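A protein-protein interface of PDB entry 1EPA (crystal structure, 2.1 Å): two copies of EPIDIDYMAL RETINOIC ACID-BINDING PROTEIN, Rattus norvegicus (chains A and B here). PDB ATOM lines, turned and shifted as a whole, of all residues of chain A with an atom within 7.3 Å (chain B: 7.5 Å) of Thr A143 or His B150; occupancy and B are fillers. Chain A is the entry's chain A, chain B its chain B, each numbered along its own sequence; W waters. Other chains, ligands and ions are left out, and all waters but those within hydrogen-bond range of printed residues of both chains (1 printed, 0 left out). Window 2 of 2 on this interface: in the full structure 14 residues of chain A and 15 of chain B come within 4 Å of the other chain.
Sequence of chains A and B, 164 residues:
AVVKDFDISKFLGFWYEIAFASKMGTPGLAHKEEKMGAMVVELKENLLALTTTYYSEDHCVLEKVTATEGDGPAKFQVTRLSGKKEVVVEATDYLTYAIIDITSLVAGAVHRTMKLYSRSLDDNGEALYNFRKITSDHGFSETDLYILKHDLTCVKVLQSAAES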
ATOM      1  N   SER A  22     -34.285   9.894 -24.025  1.00  0.00           N
ATOM      2  CA  SER A  22     -34.689  10.590 -25.223  1.00  0.00           C
ATOM      3  C   SER A  22     -34.798   9.557 -26.304  1.00  0.00           C
ATOM      4  O   SER A  22     -34.248   8.470 -26.176  1.00  0.00           O
ATOM      5  CB  SER A  22     -33.688  11.635 -25.635  1.00  0.00           C
ATOM      6  OG  SER A  22     -32.673  11.300 -26.561  1.00  0.00           O
ATOM      7  N   ARG A 132     -37.183   5.429 -13.801  1.00  0.00           N
ATOM      8  CA  ARG A 132     -37.659   4.449 -14.755  1.00  0.00           C
ATOM      9  C   ARG A 132     -39.169   4.386 -14.843  1.00  0.00           C
ATOM     10  O   ARG A 132     -39.696   4.285 -15.950  1.00  0.00           O
ATOM     11  CB  ARG A 132     -37.101   3.044 -14.437  1.00  0.00           C
ATOM     12  CG  ARG A 132     -35.630   3.115 -14.646  1.00  0.00           C
ATOM     13  CD  ARG A 132     -34.944   1.870 -14.251  1.00  0.00           C
ATOM     14  NE  ARG A 132     -33.518   1.965 -14.526  1.00  0.00           N
ATOM     15  CZ  ARG A 132     -33.018   1.546 -15.679  1.00  0.00           C
ATOM     16  NH1 ARG A 132     -33.788   1.036 -16.631  1.00  0.00           N
ATOM     17  NH2 ARG A 132     -31.712   1.578 -15.874  1.00  0.00           N
ATOM     18  N   PHE A 140     -41.370   6.344 -22.807  1.00  0.00           N
ATOM     19  CA  PHE A 140     -40.018   6.078 -23.198  1.00  0.00           C
ATOM     20  C   PHE A 140     -39.774   4.646 -22.886  1.00  0.00           C
ATOM     21  O   PHE A 140     -40.227   4.132 -21.877  1.00  0.00           O
ATOM     22  CB  PHE A 140     -38.987   6.918 -22.400  1.00  0.00           C
ATOM     23  CG  PHE A 140     -38.888   8.361 -22.834  1.00  0.00           C
ATOM     24  CD1 PHE A 140     -38.074   8.684 -23.889  1.00  0.00           C
ATOM     25  CD2 PHE A 140     -39.623   9.329 -22.198  1.00  0.00           C
ATOM     26  CE1 PHE A 140     -38.003   9.986 -24.309  1.00  0.00           C
ATOM     27  CE2 PHE A 140     -39.538  10.618 -22.635  1.00  0.00           C
ATOM     28  CZ  PHE A 140     -38.728  10.942 -23.690  1.00  0.00           C
ATOM     29  N   SER A 141     -39.060   3.989 -23.760  1.00  0.00           N
ATOM     30  CA  SER A 141     -38.588   2.645 -23.556  1.00  0.00           C
ATOM     31  C   SER A 141     -37.369   2.564 -22.637  1.00  0.00           C
ATOM     32  O   SER A 141     -36.632   3.531 -22.518  1.00  0.00           O
ATOM     33  CB  SER A 141     -38.304   2.134 -24.944  1.00  0.00           C
ATOM     34  OG  SER A 141     -37.469   0.997 -25.073  1.00  0.00           O
ATOM     35  N   GLU A 142     -37.067   1.416 -22.025  1.00  0.00           N
ATOM     36  CA  GLU A 142     -35.821   1.183 -21.291  1.00  0.00           C
ATOM     37  C   GLU A 142     -34.600   1.418 -22.167  1.00  0.00           C
ATOM     38  O   GLU A 142     -33.548   1.825 -21.690  1.00  0.00           O
ATOM     39  CB  GLU A 142     -35.745  -0.246 -20.781  1.00  0.00           C
ATOM     40  CG  GLU A 142     -34.525  -0.461 -19.909  1.00  0.00           C
ATOM     41  CD  GLU A 142     -34.559  -1.808 -19.205  1.00  0.00           C
ATOM     42  OE1 GLU A 142     -35.519  -2.024 -18.473  1.00  0.00           O
ATOM     43  OE2 GLU A 142     -33.648  -2.620 -19.402  1.00  0.00           O
ATOM     44  N   THR A 143     -34.798   1.201 -23.458  1.00  0.00           N
ATOM     45  CA  THR A 143     -33.826   1.431 -24.505  1.00  0.00           C
ATOM     46  C   THR A 143     -33.509   2.920 -24.670  1.00  0.00           C
ATOM     47  O   THR A 143     -32.489   3.346 -25.201  1.00  0.00           O
ATOM     48  CB  THR A 143     -34.492   0.739 -25.751  1.00  0.00           C
ATOM     49  OG1 THR A 143     -34.406  -0.678 -25.490  1.00  0.00           O
ATOM     50  CG2 THR A 143     -33.888   1.113 -27.072  1.00  0.00           C
ATOM     51  N   ASP A 144     -34.450   3.749 -24.246  1.00  0.00           N
ATOM     52  CA  ASP A 144     -34.340   5.173 -24.369  1.00  0.00           C
ATOM     53  C   ASP A 144     -33.691   5.823 -23.171  1.00  0.00           C
ATOM     54  O   ASP A 144     -33.576   7.039 -23.215  1.00  0.00           O
ATOM     55  CB  ASP A 144     -35.720   5.746 -24.578  1.00  0.00           C
ATOM     56  CG  ASP A 144     -36.456   5.344 -25.869  1.00  0.00           C
ATOM     57  OD1 ASP A 144     -35.831   5.171 -26.924  1.00  0.00           O
ATOM     58  OD2 ASP A 144     -37.673   5.235 -25.821  1.00  0.00           O
ATOM     59  N   LEU A 145     -33.339   5.100 -22.099  1.00  0.00           N
ATOM     60  CA  LEU A 145     -32.703   5.670 -20.925  1.00  0.00           C
ATOM     61  C   LEU A 145     -31.181   5.547 -20.993  1.00  0.00           C
ATOM     62  O   LEU A 145     -30.671   4.491 -21.413  1.00  0.00           O
ATOM     63  CB  LEU A 145     -33.128   4.969 -19.637  1.00  0.00           C
ATOM     64  CG  LEU A 145     -34.596   4.798 -19.273  1.00  0.00           C
ATOM     65  CD1 LEU A 145     -34.719   4.728 -17.735  1.00  0.00           C
ATOM     66  CD2 LEU A 145     -35.413   5.940 -19.878  1.00  0.00           C
ATOM     67  N   TYR A 146     -30.428   6.610 -20.644  1.00  0.00           N
ATOM     68  CA  TYR A 146     -28.969   6.575 -20.645  1.00  0.00           C
ATOM     69  C   TYR A 146     -28.559   7.014 -19.268  1.00  0.00           C
ATOM     70  O   TYR A 146     -29.009   8.059 -18.813  1.00  0.00           O
ATOM     71  CB  TYR A 146     -28.352   7.542 -21.633  1.00  0.00           C
ATOM     72  CG  TYR A 146     -28.829   7.253 -23.041  1.00  0.00           C
ATOM     73  CD1 TYR A 146     -30.003   7.822 -23.487  1.00  0.00           C
ATOM     74  CD2 TYR A 146     -28.122   6.382 -23.828  1.00  0.00           C
ATOM     75  CE1 TYR A 146     -30.496   7.532 -24.732  1.00  0.00           C
ATOM     76  CE2 TYR A 146     -28.609   6.072 -25.078  1.00  0.00           C
ATOM     77  CZ  TYR A 146     -29.790   6.654 -25.505  1.00  0.00           C
ATOM     78  OH  TYR A 146     -30.283   6.330 -26.735  1.00  0.00           O
ATOM     79  N   GLU B  17     -27.263  -9.707 -20.597  1.00  0.00           N
ATOM     80  CA  GLU B  17     -26.556  -9.234 -19.418  1.00  0.00           C
ATOM     81  C   GLU B  17     -26.786  -7.726 -19.400  1.00  0.00           C
ATOM     82  O   GLU B  17     -26.326  -6.972 -20.253  1.00  0.00           O
ATOM     83  CB  GLU B  17     -25.123  -9.598 -19.564  1.00  0.00           C
ATOM     84  CG  GLU B  17     -24.292  -9.417 -18.301  1.00  0.00           C
ATOM     85  CD  GLU B  17     -22.822  -9.347 -18.673  1.00  0.00           C
ATOM     86  OE1 GLU B  17     -22.191 -10.372 -18.864  1.00  0.00           O
ATOM     87  OE2 GLU B  17     -22.323  -8.253 -18.836  1.00  0.00           O
ATOM     88  N   ILE B  18     -27.651  -7.370 -18.479  1.00  0.00           N
ATOM     89  CA  ILE B  18     -28.157  -6.038 -18.233  1.00  0.00           C
ATOM     90  C   ILE B  18     -27.199  -5.144 -17.455  1.00  0.00           C
ATOM     91  O   ILE B  18     -27.134  -3.946 -17.719  1.00  0.00           O
ATOM     92  CB  ILE B  18     -29.507  -6.218 -17.475  1.00  0.00           C
ATOM     93  CG1 ILE B  18     -30.475  -6.942 -18.390  1.00  0.00           C
ATOM     94  CG2 ILE B  18     -30.142  -4.888 -17.069  1.00  0.00           C
ATOM     95  CD1 ILE B  18     -30.843  -6.294 -19.712  1.00  0.00           C
ATOM     96  N   GLU B  33     -16.793   1.816 -26.796  1.00  0.00           N
ATOM     97  CA  GLU B  33     -18.199   1.653 -27.193  1.00  0.00           C
ATOM     98  C   GLU B  33     -18.671   0.334 -26.674  1.00  0.00           C
ATOM     99  O   GLU B  33     -18.193  -0.749 -26.994  1.00  0.00           O
ATOM    100  CB  GLU B  33     -18.550   1.615 -28.690  1.00  0.00           C
ATOM    101  CG  GLU B  33     -19.730   2.558 -28.992  1.00  0.00           C
ATOM    102  CD  GLU B  33     -21.138   2.113 -28.601  1.00  0.00           C
ATOM    103  OE1 GLU B  33     -21.406   0.911 -28.657  1.00  0.00           O
ATOM    104  OE2 GLU B  33     -21.965   2.973 -28.256  1.00  0.00           O
ATOM    105  N   GLU B  34     -19.628   0.479 -25.783  1.00  0.00           N
ATOM    106  CA  GLU B  34     -20.216  -0.664 -25.131  1.00  0.00           C
ATOM    107  C   GLU B  34     -21.279  -1.426 -25.917  1.00  0.00           C
ATOM    108  O   GLU B  34     -22.204  -0.847 -26.504  1.00  0.00           O
ATOM    109  CB  GLU B  34     -20.808  -0.207 -23.842  1.00  0.00           C
ATOM    110  CG  GLU B  34     -20.814  -1.286 -22.747  1.00  0.00           C
ATOM    111  CD  GLU B  34     -21.419  -0.684 -21.510  1.00  0.00           C
ATOM    112  OE1 GLU B  34     -22.517  -0.141 -21.655  1.00  0.00           O
ATOM    113  OE2 GLU B  34     -20.796  -0.719 -20.444  1.00  0.00           O
ATOM    114  N   LYS B  35     -21.121  -2.755 -25.853  1.00  0.00           N
ATOM    115  CA  LYS B  35     -22.042  -3.647 -26.511  1.00  0.00           C
ATOM    116  C   LYS B  35     -22.610  -4.591 -25.463  1.00  0.00           C
ATOM    117  O   LYS B  35     -21.927  -5.109 -24.562  1.00  0.00           O
ATOM    118  CB  LYS B  35     -21.333  -4.432 -27.588  1.00  0.00           C
ATOM    119  CG  LYS B  35     -20.675  -3.518 -28.557  1.00  0.00           C
ATOM    120  CD  LYS B  35     -20.728  -4.160 -29.902  1.00  0.00           C
ATOM    121  CE  LYS B  35     -19.992  -3.263 -30.922  1.00  0.00           C
ATOM    122  NZ  LYS B  35     -20.666  -1.982 -31.134  1.00  0.00           N
ATOM    123  N   MET B  36     -23.902  -4.772 -25.554  1.00  0.00           N
ATOM    124  CA  MET B  36     -24.514  -5.687 -24.659  1.00  0.00           C
ATOM    125  C   MET B  36     -24.042  -7.138 -24.782  1.00  0.00           C
ATOM    126  O   MET B  36     -23.779  -7.652 -25.877  1.00  0.00           O
ATOM    127  CB  MET B  36     -25.979  -5.581 -24.872  1.00  0.00           C
ATOM    128  CG  MET B  36     -26.444  -6.046 -23.523  1.00  0.00           C
ATOM    129  SD  MET B  36     -28.124  -5.665 -23.121  1.00  0.00           S
ATOM    130  CE  MET B  36     -28.574  -6.683 -24.478  1.00  0.00           C
ATOM    131  N   SER B 120     -35.366 -10.275 -20.538  1.00  0.00           N
ATOM    132  CA  SER B 120     -35.858  -9.287 -21.445  1.00  0.00           C
ATOM    133  C   SER B 120     -35.080  -7.998 -21.318  1.00  0.00           C
ATOM    134  O   SER B 120     -34.313  -7.709 -20.396  1.00  0.00           O
ATOM    135  CB  SER B 120     -37.314  -9.193 -21.090  1.00  0.00           C
ATOM    136  OG  SER B 120     -38.027  -8.023 -21.434  1.00  0.00           O
ATOM    137  N   LEU B 121     -35.334  -7.253 -22.393  1.00  0.00           N
ATOM    138  CA  LEU B 121     -34.793  -5.932 -22.682  1.00  0.00           C
ATOM    139  C   LEU B 121     -35.668  -4.764 -22.174  1.00  0.00           C
ATOM    140  O   LEU B 121     -35.322  -3.583 -22.309  1.00  0.00           O
ATOM    141  CB  LEU B 121     -34.566  -5.820 -24.222  1.00  0.00           C
ATOM    142  CG  LEU B 121     -34.827  -6.981 -25.240  1.00  0.00           C
ATOM    143  CD1 LEU B 121     -36.288  -7.445 -25.246  1.00  0.00           C
ATOM    144  CD2 LEU B 121     -34.526  -6.469 -26.652  1.00  0.00           C
ATOM    145  N   ASP B 122     -36.796  -5.014 -21.530  1.00  0.00           N
ATOM    146  CA  ASP B 122     -37.629  -3.970 -20.972  1.00  0.00           C
ATOM    147  C   ASP B 122     -38.215  -4.363 -19.622  1.00  0.00           C
ATOM    148  O   ASP B 122     -38.295  -5.524 -19.211  1.00  0.00           O
ATOM    149  CB  ASP B 122     -38.760  -3.630 -21.939  1.00  0.00           C
ATOM    150  CG  ASP B 122     -39.476  -4.805 -22.628  1.00  0.00           C
ATOM    151  OD1 ASP B 122     -38.966  -5.328 -23.642  1.00  0.00           O
ATOM    152  OD2 ASP B 122     -40.563  -5.176 -22.162  1.00  0.00           O
ATOM    153  N   ASN B 124     -37.022  -3.865 -16.657  1.00  0.00           N
ATOM    154  CA  ASN B 124     -35.987  -4.338 -15.747  1.00  0.00           C
ATOM    155  C   ASN B 124     -35.841  -3.409 -14.555  1.00  0.00           C
ATOM    156  O   ASN B 124     -34.860  -3.538 -13.830  1.00  0.00           O
ATOM    157  CB  ASN B 124     -34.637  -4.415 -16.404  1.00  0.00           C
ATOM    158  CG  ASN B 124     -34.573  -5.535 -17.402  1.00  0.00           C
ATOM    159  OD1 ASN B 124     -34.915  -6.669 -17.122  1.00  0.00           O
ATOM    160  ND2 ASN B 124     -34.107  -5.316 -18.612  1.00  0.00           N
ATOM    161  N   LEU B 128     -33.177  -4.006 -11.501  1.00  0.00           N
ATOM    162  CA  LEU B 128     -31.989  -3.158 -11.352  1.00  0.00           C
ATOM    163  C   LEU B 128     -31.941  -2.493 -10.000  1.00  0.00           C
ATOM    164  O   LEU B 128     -30.857  -2.349  -9.457  1.00  0.00           O
ATOM    165  CB  LEU B 128     -31.940  -2.101 -12.467  1.00  0.00           C
ATOM    166  CG  LEU B 128     -31.535  -2.647 -13.865  1.00  0.00           C
ATOM    167  CD1 LEU B 128     -32.074  -1.761 -14.986  1.00  0.00           C
ATOM    168  CD2 LEU B 128     -30.004  -2.642 -14.008  1.00  0.00           C
ATOM    169  N   ILE B 147     -24.118  -0.231 -16.364  1.00  0.00           N
ATOM    170  CA  ILE B 147     -25.401  -0.599 -16.944  1.00  0.00           C
ATOM    171  C   ILE B 147     -25.135  -0.662 -18.431  1.00  0.00           C
ATOM    172  O   ILE B 147     -24.698   0.312 -19.009  1.00  0.00           O
ATOM    173  CB  ILE B 147     -26.412   0.466 -16.603  1.00  0.00           C
ATOM    174  CG1 ILE B 147     -26.347   0.875 -15.092  1.00  0.00           C
ATOM    175  CG2 ILE B 147     -27.761  -0.092 -16.990  1.00  0.00           C
ATOM    176  CD1 ILE B 147     -26.786  -0.096 -13.965  1.00  0.00           C
ATOM    177  N   LEU B 148     -25.313  -1.769 -19.104  1.00  0.00           N
ATOM    178  CA  LEU B 148     -24.865  -1.927 -20.474  1.00  0.00           C
ATOM    179  C   LEU B 148     -25.773  -1.222 -21.466  1.00  0.00           C
ATOM    180  O   LEU B 148     -26.996  -1.170 -21.248  1.00  0.00           O
ATOM    181  CB  LEU B 148     -24.784  -3.404 -20.791  1.00  0.00           C
ATOM    182  CG  LEU B 148     -23.588  -4.134 -20.268  1.00  0.00           C
ATOM    183  CD1 LEU B 148     -23.676  -4.258 -18.779  1.00  0.00           C
ATOM    184  CD2 LEU B 148     -23.564  -5.529 -20.739  1.00  0.00           C
ATOM    185  N   LYS B 149     -25.179  -0.716 -22.548  1.00  0.00           N
ATOM    186  CA  LYS B 149     -25.871   0.021 -23.569  1.00  0.00           C
ATOM    187  C   LYS B 149     -26.607  -0.987 -24.393  1.00  0.00           C
ATOM    188  O   LYS B 149     -26.114  -2.090 -24.667  1.00  0.00           O
ATOM    189  CB  LYS B 149     -24.900   0.771 -24.473  1.00  0.00           C
ATOM    190  CG  LYS B 149     -25.577   2.005 -25.167  1.00  0.00           C
ATOM    191  CD  LYS B 149     -25.790   1.838 -26.688  1.00  0.00           C
ATOM    192  CE  LYS B 149     -26.880   2.742 -27.305  1.00  0.00           C
ATOM    193  NZ  LYS B 149     -26.483   4.145 -27.253  1.00  0.00           N
ATOM    194  N   HIS B 150     -27.767  -0.576 -24.876  1.00  0.00           N
ATOM    195  CA  HIS B 150     -28.589  -1.465 -25.650  1.00  0.00           C
ATOM    196  C   HIS B 150     -28.077  -1.633 -27.061  1.00  0.00           C
ATOM    197  O   HIS B 150     -28.891  -1.688 -27.987  1.00  0.00           O
ATOM    198  CB  HIS B 150     -30.027  -0.934 -25.651  1.00  0.00           C
ATOM    199  CG  HIS B 150     -30.810  -1.345 -24.422  1.00  0.00           C
ATOM    200  ND1 HIS B 150     -32.042  -1.857 -24.367  1.00  0.00           N
ATOM    201  CD2 HIS B 150     -30.301  -1.304 -23.154  1.00  0.00           C
ATOM    202  CE1 HIS B 150     -32.270  -2.131 -23.122  1.00  0.00           C
ATOM    203  NE2 HIS B 150     -31.224  -1.793 -22.405  1.00  0.00           N
ATOM    204  N   ASP B 151     -26.769  -1.736 -27.268  1.00  0.00           N
ATOM    205  CA  ASP B 151     -26.233  -2.006 -28.585  1.00  0.00           C
ATOM    206  C   ASP B 151     -26.213  -3.533 -28.647  1.00  0.00           C
ATOM    207  O   ASP B 151     -25.486  -4.170 -27.876  1.00  0.00           O
ATOM    208  CB  ASP B 151     -24.838  -1.427 -28.667  1.00  0.00           C
ATOM    209  CG  ASP B 151     -24.042  -1.576 -29.960  1.00  0.00           C
ATOM    210  OD1 ASP B 151     -24.485  -2.126 -30.970  1.00  0.00           O
ATOM    211  OD2 ASP B 151     -22.913  -1.105 -29.931  1.00  0.00           O
ATOM    212  N   LEU B 152     -26.988  -4.145 -29.528  1.00  0.00           N
ATOM    213  CA  LEU B 152     -27.112  -5.584 -29.572  1.00  0.00           C
ATOM    214  C   LEU B 152     -26.265  -6.154 -30.670  1.00  0.00           C
ATOM    215  O   LEU B 152     -26.644  -7.212 -31.166  1.00  0.00           O
ATOM    216  CB  LEU B 152     -28.552  -6.093 -29.851  1.00  0.00           C
ATOM    217  CG  LEU B 152     -29.908  -5.773 -29.207  1.00  0.00           C
ATOM    218  CD1 LEU B 152     -29.789  -5.502 -27.685  1.00  0.00           C
ATOM    219  CD2 LEU B 152     -30.510  -4.675 -30.071  1.00  0.00           C
ATOM    220  N   THR B 153     -25.124  -5.581 -31.082  1.00  0.00           N
ATOM    221  CA  THR B 153     -24.388  -6.215 -32.166  1.00  0.00           C
ATOM    222  C   THR B 153     -23.931  -7.611 -31.765  1.00  0.00           C
ATOM    223  O   THR B 153     -24.200  -8.562 -32.508  1.00  0.00           O
ATOM    224  CB  THR B 153     -23.183  -5.388 -32.545  1.00  0.00           C
ATOM    225  OG1 THR B 153     -23.671  -4.093 -32.775  1.00  0.00           O
ATOM    226  CG2 THR B 153     -22.506  -5.850 -33.819  1.00  0.00           C
ATOM    227  N   VAL B 155     -25.028  -9.478 -29.163  1.00  0.00           N
ATOM    228  CA  VAL B 155     -26.229 -10.217 -28.848  1.00  0.00           C
ATOM    229  C   VAL B 155     -26.798 -10.935 -30.055  1.00  0.00           C
ATOM    230  O   VAL B 155     -27.050 -12.148 -30.021  1.00  0.00           O
ATOM    231  CB  VAL B 155     -27.274  -9.230 -28.230  1.00  0.00           C
ATOM    232  CG1 VAL B 155     -28.693  -9.817 -28.073  1.00  0.00           C
ATOM    233  CG2 VAL B 155     -26.740  -8.920 -26.826  1.00  0.00           C
ATOM    234  N   LYS B 156     -26.921 -10.244 -31.172  1.00  0.00           N
ATOM    235  CA  LYS B 156     -27.572 -10.838 -32.325  1.00  0.00           C
ATOM    236  C   LYS B 156     -26.701 -11.867 -32.936  1.00  0.00           C
ATOM    237  O   LYS B 156     -27.247 -12.782 -33.556  1.00  0.00           O
ATOM    238  CB  LYS B 156     -27.891  -9.825 -33.396  1.00  0.00           C
ATOM    239  CG  LYS B 156     -28.949  -8.844 -32.884  1.00  0.00           C
ATOM    240  CD  LYS B 156     -29.265  -7.869 -34.009  1.00  0.00           C
ATOM    241  CE  LYS B 156     -28.101  -6.939 -34.340  1.00  0.00           C
ATOM    242  NZ  LYS B 156     -28.592  -5.580 -34.160  1.00  0.00           N
HETATM  243  O   HOH W   1     -31.050  -1.584 -19.631  1.00  0.00           O
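OG1 of Thr A143 is in hydrogen-bond range of ND1 of His B150 (2.9 Å).
The side-chain carboxylate (OE2) of Glu A142 lies close to the backbone carbonyl oxygen (O) of Leu B121 (3.5 Å).
The side-chain amide nitrogen of Asn B124 lies within hydrogen-bond range of the side-chain carboxylate of Glu A142.
OG of Ser A141 lies close to N of Thr A143, at 3.1 Å.
NH1 of Arg A132 lies within salt-bridge range of OE1 of Glu A142, at 3.97 Å.
OE1 of Glu B34 sits at hydrogen-bond distance from N of Lys B149, 2.9 Å away.
The side-chain hydroxyl (OG) of Ser B120 lies within hydrogen-bond range of the backbone NH (N) of Asp B122.
O of Ser B120 sits at hydrogen-bond distance from ND2 of Asn B124 (3.0 Å).
Among the printed residues, pairs that only touch across the chains: Arg A132 with Leu B128, Glu A142 with Asp B122, Glu A142 with His B150 and Tyr A146 with Lys B149.
Printed residues of chain B within 4 Å of Glu A142: Leu B121, Asp B122, Asn B124 and His B150.
Thr A143 touches one residue of chain B.
Of the printed residues of chain A, Leu B121 touches Glu A142 (3.5 Å).
Printed residues of chain A within 4 Å of Leu B128: Arg A132.
Printed residues of chain A within 4 Å of Lys B149: Tyr A146 (3.6 Å).
Of chain A, only Glu A142 (3.9 Å) and Thr A143 (2.9 Å) come within 4 Å of His B150.
Asp B151 touches none of the printed residues of chain A.
The nearest printed residue of chain A that does not touch Asn B124 is Arg A132 (5.3 Å).
Of the 20 printed residues of chain B, 6 touch a printed residue of chain A.
Printed residues of chain A that touch a printed residue of chain B: Arg A132, Glu A142, Thr A143 and Tyr A146.
Along chain A the printed residues that touch a printed residue of chain B span positions 132 to 146.
No position is printed for both chains.
Of the 7 pairs that touch across the chains among the printed residues, none has its exchanged pair printed and touching as well.
Water W1 bridges NE2 of His B150 and OE2 of Glu A142.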
